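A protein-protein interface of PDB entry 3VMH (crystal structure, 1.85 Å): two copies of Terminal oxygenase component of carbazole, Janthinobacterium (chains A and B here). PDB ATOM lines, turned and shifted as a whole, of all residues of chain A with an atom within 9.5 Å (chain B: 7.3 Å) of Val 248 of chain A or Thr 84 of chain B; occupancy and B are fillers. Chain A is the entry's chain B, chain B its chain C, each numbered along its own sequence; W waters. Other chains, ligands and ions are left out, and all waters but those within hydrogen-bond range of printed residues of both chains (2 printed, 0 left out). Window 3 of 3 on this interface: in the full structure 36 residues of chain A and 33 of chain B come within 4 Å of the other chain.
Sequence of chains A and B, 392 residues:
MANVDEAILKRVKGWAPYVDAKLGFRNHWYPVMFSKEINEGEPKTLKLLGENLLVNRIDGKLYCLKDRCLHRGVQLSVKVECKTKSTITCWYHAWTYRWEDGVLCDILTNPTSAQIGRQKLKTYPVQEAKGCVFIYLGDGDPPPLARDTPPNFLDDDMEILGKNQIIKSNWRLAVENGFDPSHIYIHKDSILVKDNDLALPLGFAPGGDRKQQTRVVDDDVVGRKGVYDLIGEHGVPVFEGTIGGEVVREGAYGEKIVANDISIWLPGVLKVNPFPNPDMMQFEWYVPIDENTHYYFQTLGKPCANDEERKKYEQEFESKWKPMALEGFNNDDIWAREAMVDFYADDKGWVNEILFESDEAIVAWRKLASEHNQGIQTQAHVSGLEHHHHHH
The side-chain hydroxyl (OH) of Tyr 185 of chain A sits at hydrogen-bond distance from the side-chain carboxylate (OE1) of Glu 81 of chain B, 2.7 Å away. NZ of Lys 188 of chain A lies within salt-bridge range of OE2 of Glu 81 of chain B (2.9 Å).
The backbone carbonyl oxygen of Glu 81 of chain B lies within hydrogen-bond range of the backbone NH of Thr 89 of chain B. O of Lys 188 of chain A lies within hydrogen-bond range of NH2 of Arg 249 of chain A (3.2 Å). The indole nitrogen (NE1) of Trp 99 of chain B lies within hydrogen-bond range of the backbone carbonyl oxygen (O) of Thr 87 of chain B (3.4 Å). OG1 of Thr 84 of chain B lies within hydrogen-bond range of OG1 of Thr 87 of chain B. N of Val 248 of chain A lies within hydrogen-bond range of O of Gly 241 of chain A. OG1 of Thr 89 of chain B sits at hydrogen-bond distance from OG1 of Thr 96 of chain B (2.8 Å).
OH of Tyr 185 of chain A touches CE of Lys 83 of chain B, at 2.9 Å. OH of Tyr 185 of chain A touches CG2 of Thr 89 of chain B, 3.9 Å away. Leu 108 of chain B touches Tyr 185 of chain A (CD2 to OH, 3.9 Å). Thr 242 of chain A touches Leu 108 of chain B. CB of Lys 83 of chain B touches CD1 of Ile 243 of chain A, 3.6 Å away. Thr 87 of chain B touches Ile 243 of chain A. Ile 243 of chain A touches Thr 89 of chain B (CD1 to OG1, 3.7 Å). Ile 243 of chain A touches Leu 108 of chain B (CG1 to CD1, 3.96 Å). Lys 83 of chain B touches Val 248 of chain A. Val 248 of chain A touches Thr 84 of chain B.
Of the printed residues of chain B, Val 248 of chain A touches Lys 83 (3.6 Å) and Thr 84 (3.9 Å). Thr 84 of chain B touches two residues of chain A. Of chain A, only Tyr 185 (2.9 Å), Ile 243 (3.6 Å) and Val 248 (3.6 Å) come within 4 Å of Lys 83 of chain B. No residue of chain A comes within 4 Å of Ser 86 of chain B. Printed residues of chain B within 4 Å of Ile 243 of chain A: Lys 83 (3.6 Å), Thr 84 (3.6 Å), Thr 87 (3.9 Å), Thr 89 (3.7 Å) and Leu 108 (3.96 Å). Printed residues of chain A within 4 Å of Leu 108 of chain B: Tyr 185 (3.9 Å), Thr 242 (3.7 Å) and Ile 243 (3.96 Å).
Hydrophobic or aromatic side chains of chain A that line the printed part of chain B: Tyr 185, Ile 243 and Val 248. Of the 16 printed residues of chain B, 6 touch a printed residue of chain A. Hydrophobic or aromatic side chains of chain B that line the printed part of chain A: Leu 108. Among the printed residues, 13 pairs touch across the chains.
No position is printed for both chains.
Water W2 bridges NZ of Lys 83 of chain B (2.7 Å) and NH1 of Arg 249 of chain A (3.0 Å). Water W1 lies within hydrogen-bond range of the side-chain amino group of Lys 188 of chain A (2.8 Å) and the side-chain carboxylate of Glu 81 of chain B (3.0 Å).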
ATOM      1  N   TYR A 185       6.850  -4.049  12.872  1.00  0.00           N
ATOM      2  CA  TYR A 185       7.790  -2.981  13.187  1.00  0.00           C
ATOM      3  C   TYR A 185       7.703  -2.529  14.650  1.00  0.00           C
ATOM      4  O   TYR A 185       8.714  -2.144  15.243  1.00  0.00           O
ATOM      5  CB  TYR A 185       7.527  -1.787  12.265  1.00  0.00           C
ATOM      6  CG  TYR A 185       8.496  -0.640  12.439  1.00  0.00           C
ATOM      7  CD1 TYR A 185       9.794  -0.718  11.939  1.00  0.00           C
ATOM      8  CD2 TYR A 185       8.124   0.514  13.132  1.00  0.00           C
ATOM      9  CE1 TYR A 185      10.703   0.325  12.121  1.00  0.00           C
ATOM     10  CE2 TYR A 185       9.024   1.560  13.322  1.00  0.00           C
ATOM     11  CZ  TYR A 185      10.312   1.459  12.814  1.00  0.00           C
ATOM     12  OH  TYR A 185      11.213   2.486  13.006  1.00  0.00           O
ATOM     13  N   LYS A 188      10.035  -4.546  17.174  1.00  0.00           N
ATOM     14  CA  LYS A 188      11.486  -4.577  16.999  1.00  0.00           C
ATOM     15  C   LYS A 188      12.315  -4.506  18.280  1.00  0.00           C
ATOM     16  O   LYS A 188      13.447  -4.990  18.307  1.00  0.00           O
ATOM     17  CB  LYS A 188      11.924  -3.472  16.030  1.00  0.00           C
ATOM     18  CG  LYS A 188      11.581  -2.057  16.464  1.00  0.00           C
ATOM     19  CD  LYS A 188      11.924  -1.055  15.370  1.00  0.00           C
ATOM     20  CE  LYS A 188      11.665   0.383  15.815  1.00  0.00           C
ATOM     21  NZ  LYS A 188      10.226   0.601  16.155  1.00  0.00           N
ATOM     22  N   ASP A 189      11.762  -3.924  19.342  1.00  0.00           N
ATOM     23  CA  ASP A 189      12.494  -3.816  20.603  1.00  0.00           C
ATOM     24  C   ASP A 189      11.951  -4.715  21.703  1.00  0.00           C
ATOM     25  O   ASP A 189      12.350  -4.591  22.860  1.00  0.00           O
ATOM     26  CB  ASP A 189      12.503  -2.369  21.104  1.00  0.00           C
ATOM     27  CG  ASP A 189      13.242  -1.436  20.176  1.00  0.00           C
ATOM     28  OD1 ASP A 189      14.359  -1.794  19.748  1.00  0.00           O
ATOM     29  OD2 ASP A 189      12.715  -0.340  19.880  1.00  0.00           O
ATOM     30  N   LEU A 202      11.838  -6.075   9.775  1.00  0.00           N
ATOM     31  CA  LEU A 202      11.184  -4.820  10.127  1.00  0.00           C
ATOM     32  C   LEU A 202       9.924  -4.668   9.290  1.00  0.00           C
ATOM     33  O   LEU A 202       9.009  -3.927   9.643  1.00  0.00           O
ATOM     34  CB  LEU A 202      12.114  -3.645   9.839  1.00  0.00           C
ATOM     35  CG  LEU A 202      13.452  -3.608  10.572  1.00  0.00           C
ATOM     36  CD1 LEU A 202      14.292  -2.458  10.023  1.00  0.00           C
ATOM     37  CD2 LEU A 202      13.218  -3.450  12.068  1.00  0.00           C
ATOM     38  N   PHE A 239      15.415  -6.148   6.497  1.00  0.00           N
ATOM     39  CA  PHE A 239      16.237  -6.279   7.692  1.00  0.00           C
ATOM     40  C   PHE A 239      17.093  -5.036   7.915  1.00  0.00           C
ATOM     41  O   PHE A 239      17.728  -4.890   8.956  1.00  0.00           O
ATOM     42  CB  PHE A 239      17.113  -7.533   7.599  1.00  0.00           C
ATOM     43  CG  PHE A 239      16.435  -8.775   8.102  1.00  0.00           C
ATOM     44  CD1 PHE A 239      16.358  -9.036   9.467  1.00  0.00           C
ATOM     45  CD2 PHE A 239      15.842  -9.670   7.217  1.00  0.00           C
ATOM     46  CE1 PHE A 239      15.704 -10.168   9.945  1.00  0.00           C
ATOM     47  CE2 PHE A 239      15.183 -10.807   7.685  1.00  0.00           C
ATOM     48  CZ  PHE A 239      15.115 -11.055   9.052  1.00  0.00           C
ATOM     49  N   GLU A 240      17.100  -4.142   6.933  1.00  0.00           N
ATOM     50  CA  GLU A 240      17.851  -2.893   7.026  1.00  0.00           C
ATOM     51  C   GLU A 240      16.963  -1.733   6.603  1.00  0.00           C
ATOM     52  O   GLU A 240      16.750  -1.507   5.410  1.00  0.00           O
ATOM     53  CB  GLU A 240      19.094  -2.931   6.131  1.00  0.00           C
ATOM     54  CG  GLU A 240      20.174  -3.886   6.608  1.00  0.00           C
ATOM     55  CD  GLU A 240      21.427  -3.812   5.761  1.00  0.00           C
ATOM     56  OE1 GLU A 240      22.028  -2.719   5.673  1.00  0.00           O
ATOM     57  OE2 GLU A 240      21.814  -4.848   5.182  1.00  0.00           O
ATOM     58  N   GLY A 241      16.437  -1.006   7.585  1.00  0.00           N
ATOM     59  CA  GLY A 241      15.581   0.127   7.286  1.00  0.00           C
ATOM     60  C   GLY A 241      16.407   1.356   6.970  1.00  0.00           C
ATOM     61  O   GLY A 241      17.327   1.702   7.715  1.00  0.00           O
ATOM     62  N   THR A 242      16.078   2.025   5.872  1.00  0.00           N
ATOM     63  CA  THR A 242      16.819   3.205   5.462  1.00  0.00           C
ATOM     64  C   THR A 242      15.983   4.461   5.262  1.00  0.00           C
ATOM     65  O   THR A 242      14.785   4.408   4.977  1.00  0.00           O
ATOM     66  CB  THR A 242      17.562   2.965   4.139  1.00  0.00           C
ATOM     67  OG1 THR A 242      16.604   2.816   3.082  1.00  0.00           O
ATOM     68  CG2 THR A 242      18.423   1.712   4.226  1.00  0.00           C
ATOM     69  N   ILE A 243      16.656   5.594   5.415  1.00  0.00           N
ATOM     70  CA  ILE A 243      16.066   6.906   5.224  1.00  0.00           C
ATOM     71  C   ILE A 243      17.107   7.644   4.398  1.00  0.00           C
ATOM     72  O   ILE A 243      18.254   7.781   4.822  1.00  0.00           O
ATOM     73  CB  ILE A 243      15.847   7.639   6.565  1.00  0.00           C
ATOM     74  CG1 ILE A 243      14.793   6.896   7.395  1.00  0.00           C
ATOM     75  CG2 ILE A 243      15.421   9.067   6.307  1.00  0.00           C
ATOM     76  CD1 ILE A 243      14.539   7.502   8.766  1.00  0.00           C
ATOM     77  N   GLY A 244      16.717   8.098   3.214  1.00  0.00           N
ATOM     78  CA  GLY A 244      17.663   8.791   2.363  1.00  0.00           C
ATOM     79  C   GLY A 244      18.807   7.871   1.973  1.00  0.00           C
ATOM     80  O   GLY A 244      19.925   8.325   1.729  1.00  0.00           O
ATOM     81  N   GLY A 245      18.529   6.570   1.927  1.00  0.00           N
ATOM     82  CA  GLY A 245      19.550   5.604   1.558  1.00  0.00           C
ATOM     83  C   GLY A 245      20.465   5.196   2.697  1.00  0.00           C
ATOM     84  O   GLY A 245      21.270   4.279   2.549  1.00  0.00           O
ATOM     85  N   GLU A 246      20.340   5.874   3.835  1.00  0.00           N
ATOM     86  CA  GLU A 246      21.163   5.580   5.005  1.00  0.00           C
ATOM     87  C   GLU A 246      20.456   4.617   5.953  1.00  0.00           C
ATOM     88  O   GLU A 246      19.295   4.818   6.301  1.00  0.00           O
ATOM     89  CB  GLU A 246      21.485   6.877   5.750  1.00  0.00           C
ATOM     90  CG  GLU A 246      22.964   7.206   5.822  1.00  0.00           C
ATOM     91  CD  GLU A 246      23.628   7.211   4.459  1.00  0.00           C
ATOM     92  OE1 GLU A 246      23.179   7.975   3.576  1.00  0.00           O
ATOM     93  OE2 GLU A 246      24.602   6.448   4.275  1.00  0.00           O
ATOM     94  N   VAL A 247      21.158   3.570   6.372  1.00  0.00           N
ATOM     95  CA  VAL A 247      20.578   2.595   7.283  1.00  0.00           C
ATOM     96  C   VAL A 247      20.421   3.231   8.659  1.00  0.00           C
ATOM     97  O   VAL A 247      21.389   3.716   9.240  1.00  0.00           O
ATOM     98  CB  VAL A 247      21.467   1.334   7.393  1.00  0.00           C
ATOM     99  CG1 VAL A 247      20.877   0.355   8.401  1.00  0.00           C
ATOM    100  CG2 VAL A 247      21.590   0.676   6.030  1.00  0.00           C
ATOM    101  N   VAL A 248      19.194   3.234   9.173  1.00  0.00           N
ATOM    102  CA  VAL A 248      18.917   3.818  10.479  1.00  0.00           C
ATOM    103  C   VAL A 248      18.376   2.789  11.457  1.00  0.00           C
ATOM    104  O   VAL A 248      18.256   3.058  12.650  1.00  0.00           O
ATOM    105  CB  VAL A 248      17.902   4.975  10.367  1.00  0.00           C
ATOM    106  CG1 VAL A 248      18.464   6.070   9.481  1.00  0.00           C
ATOM    107  CG2 VAL A 248      16.580   4.457   9.804  1.00  0.00           C
ATOM    108  N   ARG A 249      18.038   1.607  10.954  1.00  0.00           N
ATOM    109  CA  ARG A 249      17.511   0.555  11.811  1.00  0.00           C
ATOM    110  C   ARG A 249      17.684  -0.820  11.185  1.00  0.00           C
ATOM    111  O   ARG A 249      17.561  -0.980   9.973  1.00  0.00           O
ATOM    112  CB  ARG A 249      16.025   0.786  12.101  1.00  0.00           C
ATOM    113  CG  ARG A 249      15.389  -0.321  12.937  1.00  0.00           C
ATOM    114  CD  ARG A 249      15.776  -0.222  14.404  1.00  0.00           C
ATOM    115  NE  ARG A 249      15.641  -1.500  15.103  1.00  0.00           N
ATOM    116  CZ  ARG A 249      15.411  -1.619  16.406  1.00  0.00           C
ATOM    117  NH1 ARG A 249      15.275  -0.535  17.161  1.00  0.00           N
ATOM    118  NH2 ARG A 249      15.329  -2.818  16.962  1.00  0.00           N
ATOM    119  N   GLU A 250      17.969  -1.810  12.021  1.00  0.00           N
ATOM    120  CA  GLU A 250      18.140  -3.175  11.545  1.00  0.00           C
ATOM    121  C   GLU A 250      17.155  -4.110  12.228  1.00  0.00           C
ATOM    122  O   GLU A 250      16.768  -3.891  13.378  1.00  0.00           O
ATOM    123  CB  GLU A 250      19.565  -3.669  11.817  1.00  0.00           C
ATOM    124  CG  GLU A 250      20.640  -2.965  11.015  1.00  0.00           C
ATOM    125  CD  GLU A 250      22.008  -3.586  11.224  1.00  0.00           C
ATOM    126  OE1 GLU A 250      22.520  -3.524  12.362  1.00  0.00           O
ATOM    127  OE2 GLU A 250      22.565  -4.141  10.251  1.00  0.00           O
ATOM    128  N   GLY A 251      16.748  -5.151  11.511  1.00  0.00           N
ATOM    129  CA  GLY A 251      15.835  -6.124  12.080  1.00  0.00           C
ATOM    130  C   GLY A 251      16.632  -7.013  13.012  1.00  0.00           C
ATOM    131  O   GLY A 251      17.794  -6.718  13.293  1.00  0.00           O
ATOM    132  N   ASN B  56       8.659  21.036  16.279  1.00  0.00           N
ATOM    133  CA  ASN B  56      10.023  20.628  16.563  1.00  0.00           C
ATOM    134  C   ASN B  56      10.977  21.727  16.122  1.00  0.00           C
ATOM    135  O   ASN B  56      10.650  22.527  15.249  1.00  0.00           O
ATOM    136  CB  ASN B  56      10.329  19.325  15.817  1.00  0.00           C
ATOM    137  CG  ASN B  56      11.645  18.695  16.240  1.00  0.00           C
ATOM    138  OD1 ASN B  56      12.122  18.895  17.359  1.00  0.00           O
ATOM    139  ND2 ASN B  56      12.226  17.901  15.346  1.00  0.00           N
ATOM    140  N   ILE B  58      14.661  22.323  14.535  1.00  0.00           N
ATOM    141  CA  ILE B  58      15.759  21.673  13.828  1.00  0.00           C
ATOM    142  C   ILE B  58      16.746  22.733  13.342  1.00  0.00           C
ATOM    143  O   ILE B  58      16.405  23.587  12.519  1.00  0.00           O
ATOM    144  CB  ILE B  58      15.234  20.873  12.622  1.00  0.00           C
ATOM    145  CG1 ILE B  58      14.162  19.882  13.087  1.00  0.00           C
ATOM    146  CG2 ILE B  58      16.384  20.131  11.938  1.00  0.00           C
ATOM    147  CD1 ILE B  58      13.541  19.086  11.955  1.00  0.00           C
ATOM    148  N   GLU B  81       9.724   8.839  16.964  1.00  0.00           N
ATOM    149  CA  GLU B  81      10.915   8.215  16.404  1.00  0.00           C
ATOM    150  C   GLU B  81      11.540   9.116  15.350  1.00  0.00           C
ATOM    151  O   GLU B  81      11.186   9.046  14.174  1.00  0.00           O
ATOM    152  CB  GLU B  81      10.588   6.850  15.776  1.00  0.00           C
ATOM    153  CG  GLU B  81      10.352   5.731  16.783  1.00  0.00           C
ATOM    154  CD  GLU B  81      10.295   4.353  16.133  1.00  0.00           C
ATOM    155  OE1 GLU B  81      10.806   4.198  15.006  1.00  0.00           O
ATOM    156  OE2 GLU B  81       9.756   3.419  16.760  1.00  0.00           O
ATOM    157  N   CYS B  82      12.454   9.981  15.772  1.00  0.00           N
ATOM    158  CA  CYS B  82      13.135  10.855  14.830  1.00  0.00           C
ATOM    159  C   CYS B  82      14.474  10.190  14.523  1.00  0.00           C
ATOM    160  O   CYS B  82      15.487  10.472  15.163  1.00  0.00           O
ATOM    161  CB  CYS B  82      13.339  12.247  15.436  1.00  0.00           C
ATOM    162  SG  CYS B  82      11.789  13.175  15.627  1.00  0.00           S
ATOM    163  N   LYS B  83      14.461   9.292  13.543  1.00  0.00           N
ATOM    164  CA  LYS B  83      15.651   8.542  13.159  1.00  0.00           C
ATOM    165  C   LYS B  83      16.728   9.357  12.462  1.00  0.00           C
ATOM    166  O   LYS B  83      17.896   8.974  12.467  1.00  0.00           O
ATOM    167  CB  LYS B  83      15.246   7.338  12.311  1.00  0.00           C
ATOM    168  CG  LYS B  83      14.287   6.422  13.051  1.00  0.00           C
ATOM    169  CD  LYS B  83      14.385   4.990  12.572  1.00  0.00           C
ATOM    170  CE  LYS B  83      13.624   4.073  13.505  1.00  0.00           C
ATOM    171  NZ  LYS B  83      14.050   4.244  14.923  1.00  0.00           N
ATOM    172  N   THR B  84      16.339  10.460  11.837  1.00  0.00           N
ATOM    173  CA  THR B  84      17.308  11.343  11.209  1.00  0.00           C
ATOM    174  C   THR B  84      16.917  12.742  11.659  1.00  0.00           C
ATOM    175  O   THR B  84      15.798  12.965  12.130  1.00  0.00           O
ATOM    176  CB  THR B  84      17.307  11.269   9.660  1.00  0.00           C
ATOM    177  OG1 THR B  84      16.100  11.833   9.139  1.00  0.00           O
ATOM    178  CG2 THR B  84      17.453   9.828   9.197  1.00  0.00           C
ATOM    179  N   LYS B  85      17.845  13.678  11.520  1.00  0.00           N
ATOM    180  CA  LYS B  85      17.627  15.054  11.943  1.00  0.00           C
ATOM    181  C   LYS B  85      16.481  15.778  11.235  1.00  0.00           C
ATOM    182  O   LYS B  85      15.777  16.579  11.851  1.00  0.00           O
ATOM    183  CB  LYS B  85      18.927  15.829  11.756  1.00  0.00           C
ATOM    184  CG  LYS B  85      19.012  17.149  12.478  1.00  0.00           C
ATOM    185  CD  LYS B  85      20.417  17.703  12.307  1.00  0.00           C
ATOM    186  CE  LYS B  85      20.593  19.040  12.980  1.00  0.00           C
ATOM    187  NZ  LYS B  85      21.970  19.549  12.743  1.00  0.00           N
ATOM    188  N   SER B  86      16.286  15.489   9.952  1.00  0.00           N
ATOM    189  CA  SER B  86      15.245  16.147   9.168  1.00  0.00           C
ATOM    190  C   SER B  86      13.943  15.362   9.000  1.00  0.00           C
ATOM    191  O   SER B  86      13.079  15.764   8.221  1.00  0.00           O
ATOM    192  CB  SER B  86      15.783  16.477   7.778  1.00  0.00           C
ATOM    193  OG  SER B  86      16.036  15.285   7.051  1.00  0.00           O
ATOM    194  N   THR B  87      13.790  14.260   9.719  1.00  0.00           N
ATOM    195  CA  THR B  87      12.572  13.467   9.563  1.00  0.00           C
ATOM    196  C   THR B  87      12.021  12.890  10.852  1.00  0.00           C
ATOM    197  O   THR B  87      12.664  12.927  11.898  1.00  0.00           O
ATOM    198  CB  THR B  87      12.800  12.274   8.588  1.00  0.00           C
ATOM    199  OG1 THR B  87      13.689  11.329   9.191  1.00  0.00           O
ATOM    200  CG2 THR B  87      13.402  12.749   7.277  1.00  0.00           C
ATOM    201  N   ILE B  88      10.803  12.360  10.760  1.00  0.00           N
ATOM    202  CA  ILE B  88      10.159  11.703  11.883  1.00  0.00           C
ATOM    203  C   ILE B  88       9.533  10.440  11.303  1.00  0.00           C
ATOM    204  O   ILE B  88       8.929  10.473  10.229  1.00  0.00           O
ATOM    205  CB  ILE B  88       9.062  12.582  12.550  1.00  0.00           C
ATOM    206  CG1 ILE B  88       8.415  11.799  13.696  1.00  0.00           C
ATOM    207  CG2 ILE B  88       8.024  13.009  11.529  1.00  0.00           C
ATOM    208  CD1 ILE B  88       7.499  12.621  14.596  1.00  0.00           C
ATOM    209  N   THR B  89       9.698   9.331  12.011  1.00  0.00           N
ATOM    210  CA  THR B  89       9.180   8.039  11.563  1.00  0.00           C
ATOM    211  C   THR B  89       8.038   7.549  12.439  1.00  0.00           C
ATOM    212  O   THR B  89       8.202   7.397  13.649  1.00  0.00           O
ATOM    213  CB  THR B  89      10.309   6.978  11.574  1.00  0.00           C
ATOM    214  OG1 THR B  89      11.303   7.336  10.608  1.00  0.00           O
ATOM    215  CG2 THR B  89       9.761   5.591  11.252  1.00  0.00           C
ATOM    216  N   THR B  96       7.801   7.532   6.906  1.00  0.00           N
ATOM    217  CA  THR B  96       8.685   8.623   7.301  1.00  0.00           C
ATOM    218  C   THR B  96       8.444   9.922   6.550  1.00  0.00           C
ATOM    219  O   THR B  96       8.398   9.951   5.322  1.00  0.00           O
ATOM    220  CB  THR B  96      10.148   8.164   7.143  1.00  0.00           C
ATOM    221  OG1 THR B  96      10.351   6.998   7.953  1.00  0.00           O
ATOM    222  CG2 THR B  96      11.124   9.258   7.578  1.00  0.00           C
ATOM    223  N   TYR B  97       8.296  11.008   7.303  1.00  0.00           N
ATOM    224  CA  TYR B  97       8.033  12.314   6.720  1.00  0.00           C
ATOM    225  C   TYR B  97       9.128  13.327   7.027  1.00  0.00           C
ATOM    226  O   TYR B  97       9.771  13.265   8.072  1.00  0.00           O
ATOM    227  CB  TYR B  97       6.711  12.881   7.247  1.00  0.00           C
ATOM    228  CG  TYR B  97       5.554  11.907   7.270  1.00  0.00           C
ATOM    229  CD1 TYR B  97       5.382  11.023   8.332  1.00  0.00           C
ATOM    230  CD2 TYR B  97       4.622  11.884   6.235  1.00  0.00           C
ATOM    231  CE1 TYR B  97       4.306  10.137   8.368  1.00  0.00           C
ATOM    232  CE2 TYR B  97       3.543  11.006   6.259  1.00  0.00           C
ATOM    233  CZ  TYR B  97       3.392  10.138   7.327  1.00  0.00           C
ATOM    234  OH  TYR B  97       2.313   9.285   7.352  1.00  0.00           O
ATOM    235  N   TRP B  99      10.263  16.966   8.096  1.00  0.00           N
ATOM    236  CA  TRP B  99       9.696  18.078   8.854  1.00  0.00           C
ATOM    237  C   TRP B  99       9.541  19.313   7.978  1.00  0.00           C
ATOM    238  O   TRP B  99       8.616  20.100   8.153  1.00  0.00           O
ATOM    239  CB  TRP B  99      10.585  18.439  10.049  1.00  0.00           C
ATOM    240  CG  TRP B  99      10.517  17.487  11.190  1.00  0.00           C
ATOM    241  CD1 TRP B  99      11.373  16.455  11.454  1.00  0.00           C
ATOM    242  CD2 TRP B  99       9.552  17.491  12.250  1.00  0.00           C
ATOM    243  NE1 TRP B  99      11.003  15.819  12.619  1.00  0.00           N
ATOM    244  CE2 TRP B  99       9.888  16.437  13.125  1.00  0.00           C
ATOM    245  CE3 TRP B  99       8.436  18.290  12.544  1.00  0.00           C
ATOM    246  CZ2 TRP B  99       9.148  16.155  14.279  1.00  0.00           C
ATOM    247  CZ3 TRP B  99       7.699  18.010  13.692  1.00  0.00           C
ATOM    248  CH2 TRP B  99       8.059  16.951  14.545  1.00  0.00           C
ATOM    249  N   CYS B 105       8.802  10.615   2.565  1.00  0.00           N
ATOM    250  CA  CYS B 105      10.052  10.351   1.851  1.00  0.00           C
ATOM    251  C   CYS B 105      10.593   8.927   1.919  1.00  0.00           C
ATOM    252  O   CYS B 105      11.451   8.555   1.115  1.00  0.00           O
ATOM    253  CB  CYS B 105      11.134  11.312   2.354  1.00  0.00           C
ATOM    254  SG  CYS B 105      11.607  11.014   4.069  1.00  0.00           S
ATOM    255  N   LEU B 108      10.129   2.456   6.043  1.00  0.00           N
ATOM    256  CA  LEU B 108      11.022   1.383   6.453  1.00  0.00           C
ATOM    257  C   LEU B 108      10.457  -0.027   6.342  1.00  0.00           C
ATOM    258  O   LEU B 108      11.209  -0.976   6.120  1.00  0.00           O
ATOM    259  CB  LEU B 108      11.523   1.635   7.877  1.00  0.00           C
ATOM    260  CG  LEU B 108      12.554   2.765   8.038  1.00  0.00           C
ATOM    261  CD1 LEU B 108      12.023   4.061   7.463  1.00  0.00           C
ATOM    262  CD2 LEU B 108      12.885   2.938   9.505  1.00  0.00           C
HETATM  263  O   HOH W   1       7.625   1.321  17.042  1.00  0.00           O
HETATM  264  O   HOH W   2      15.152   2.391  16.610  1.00  0.00           O
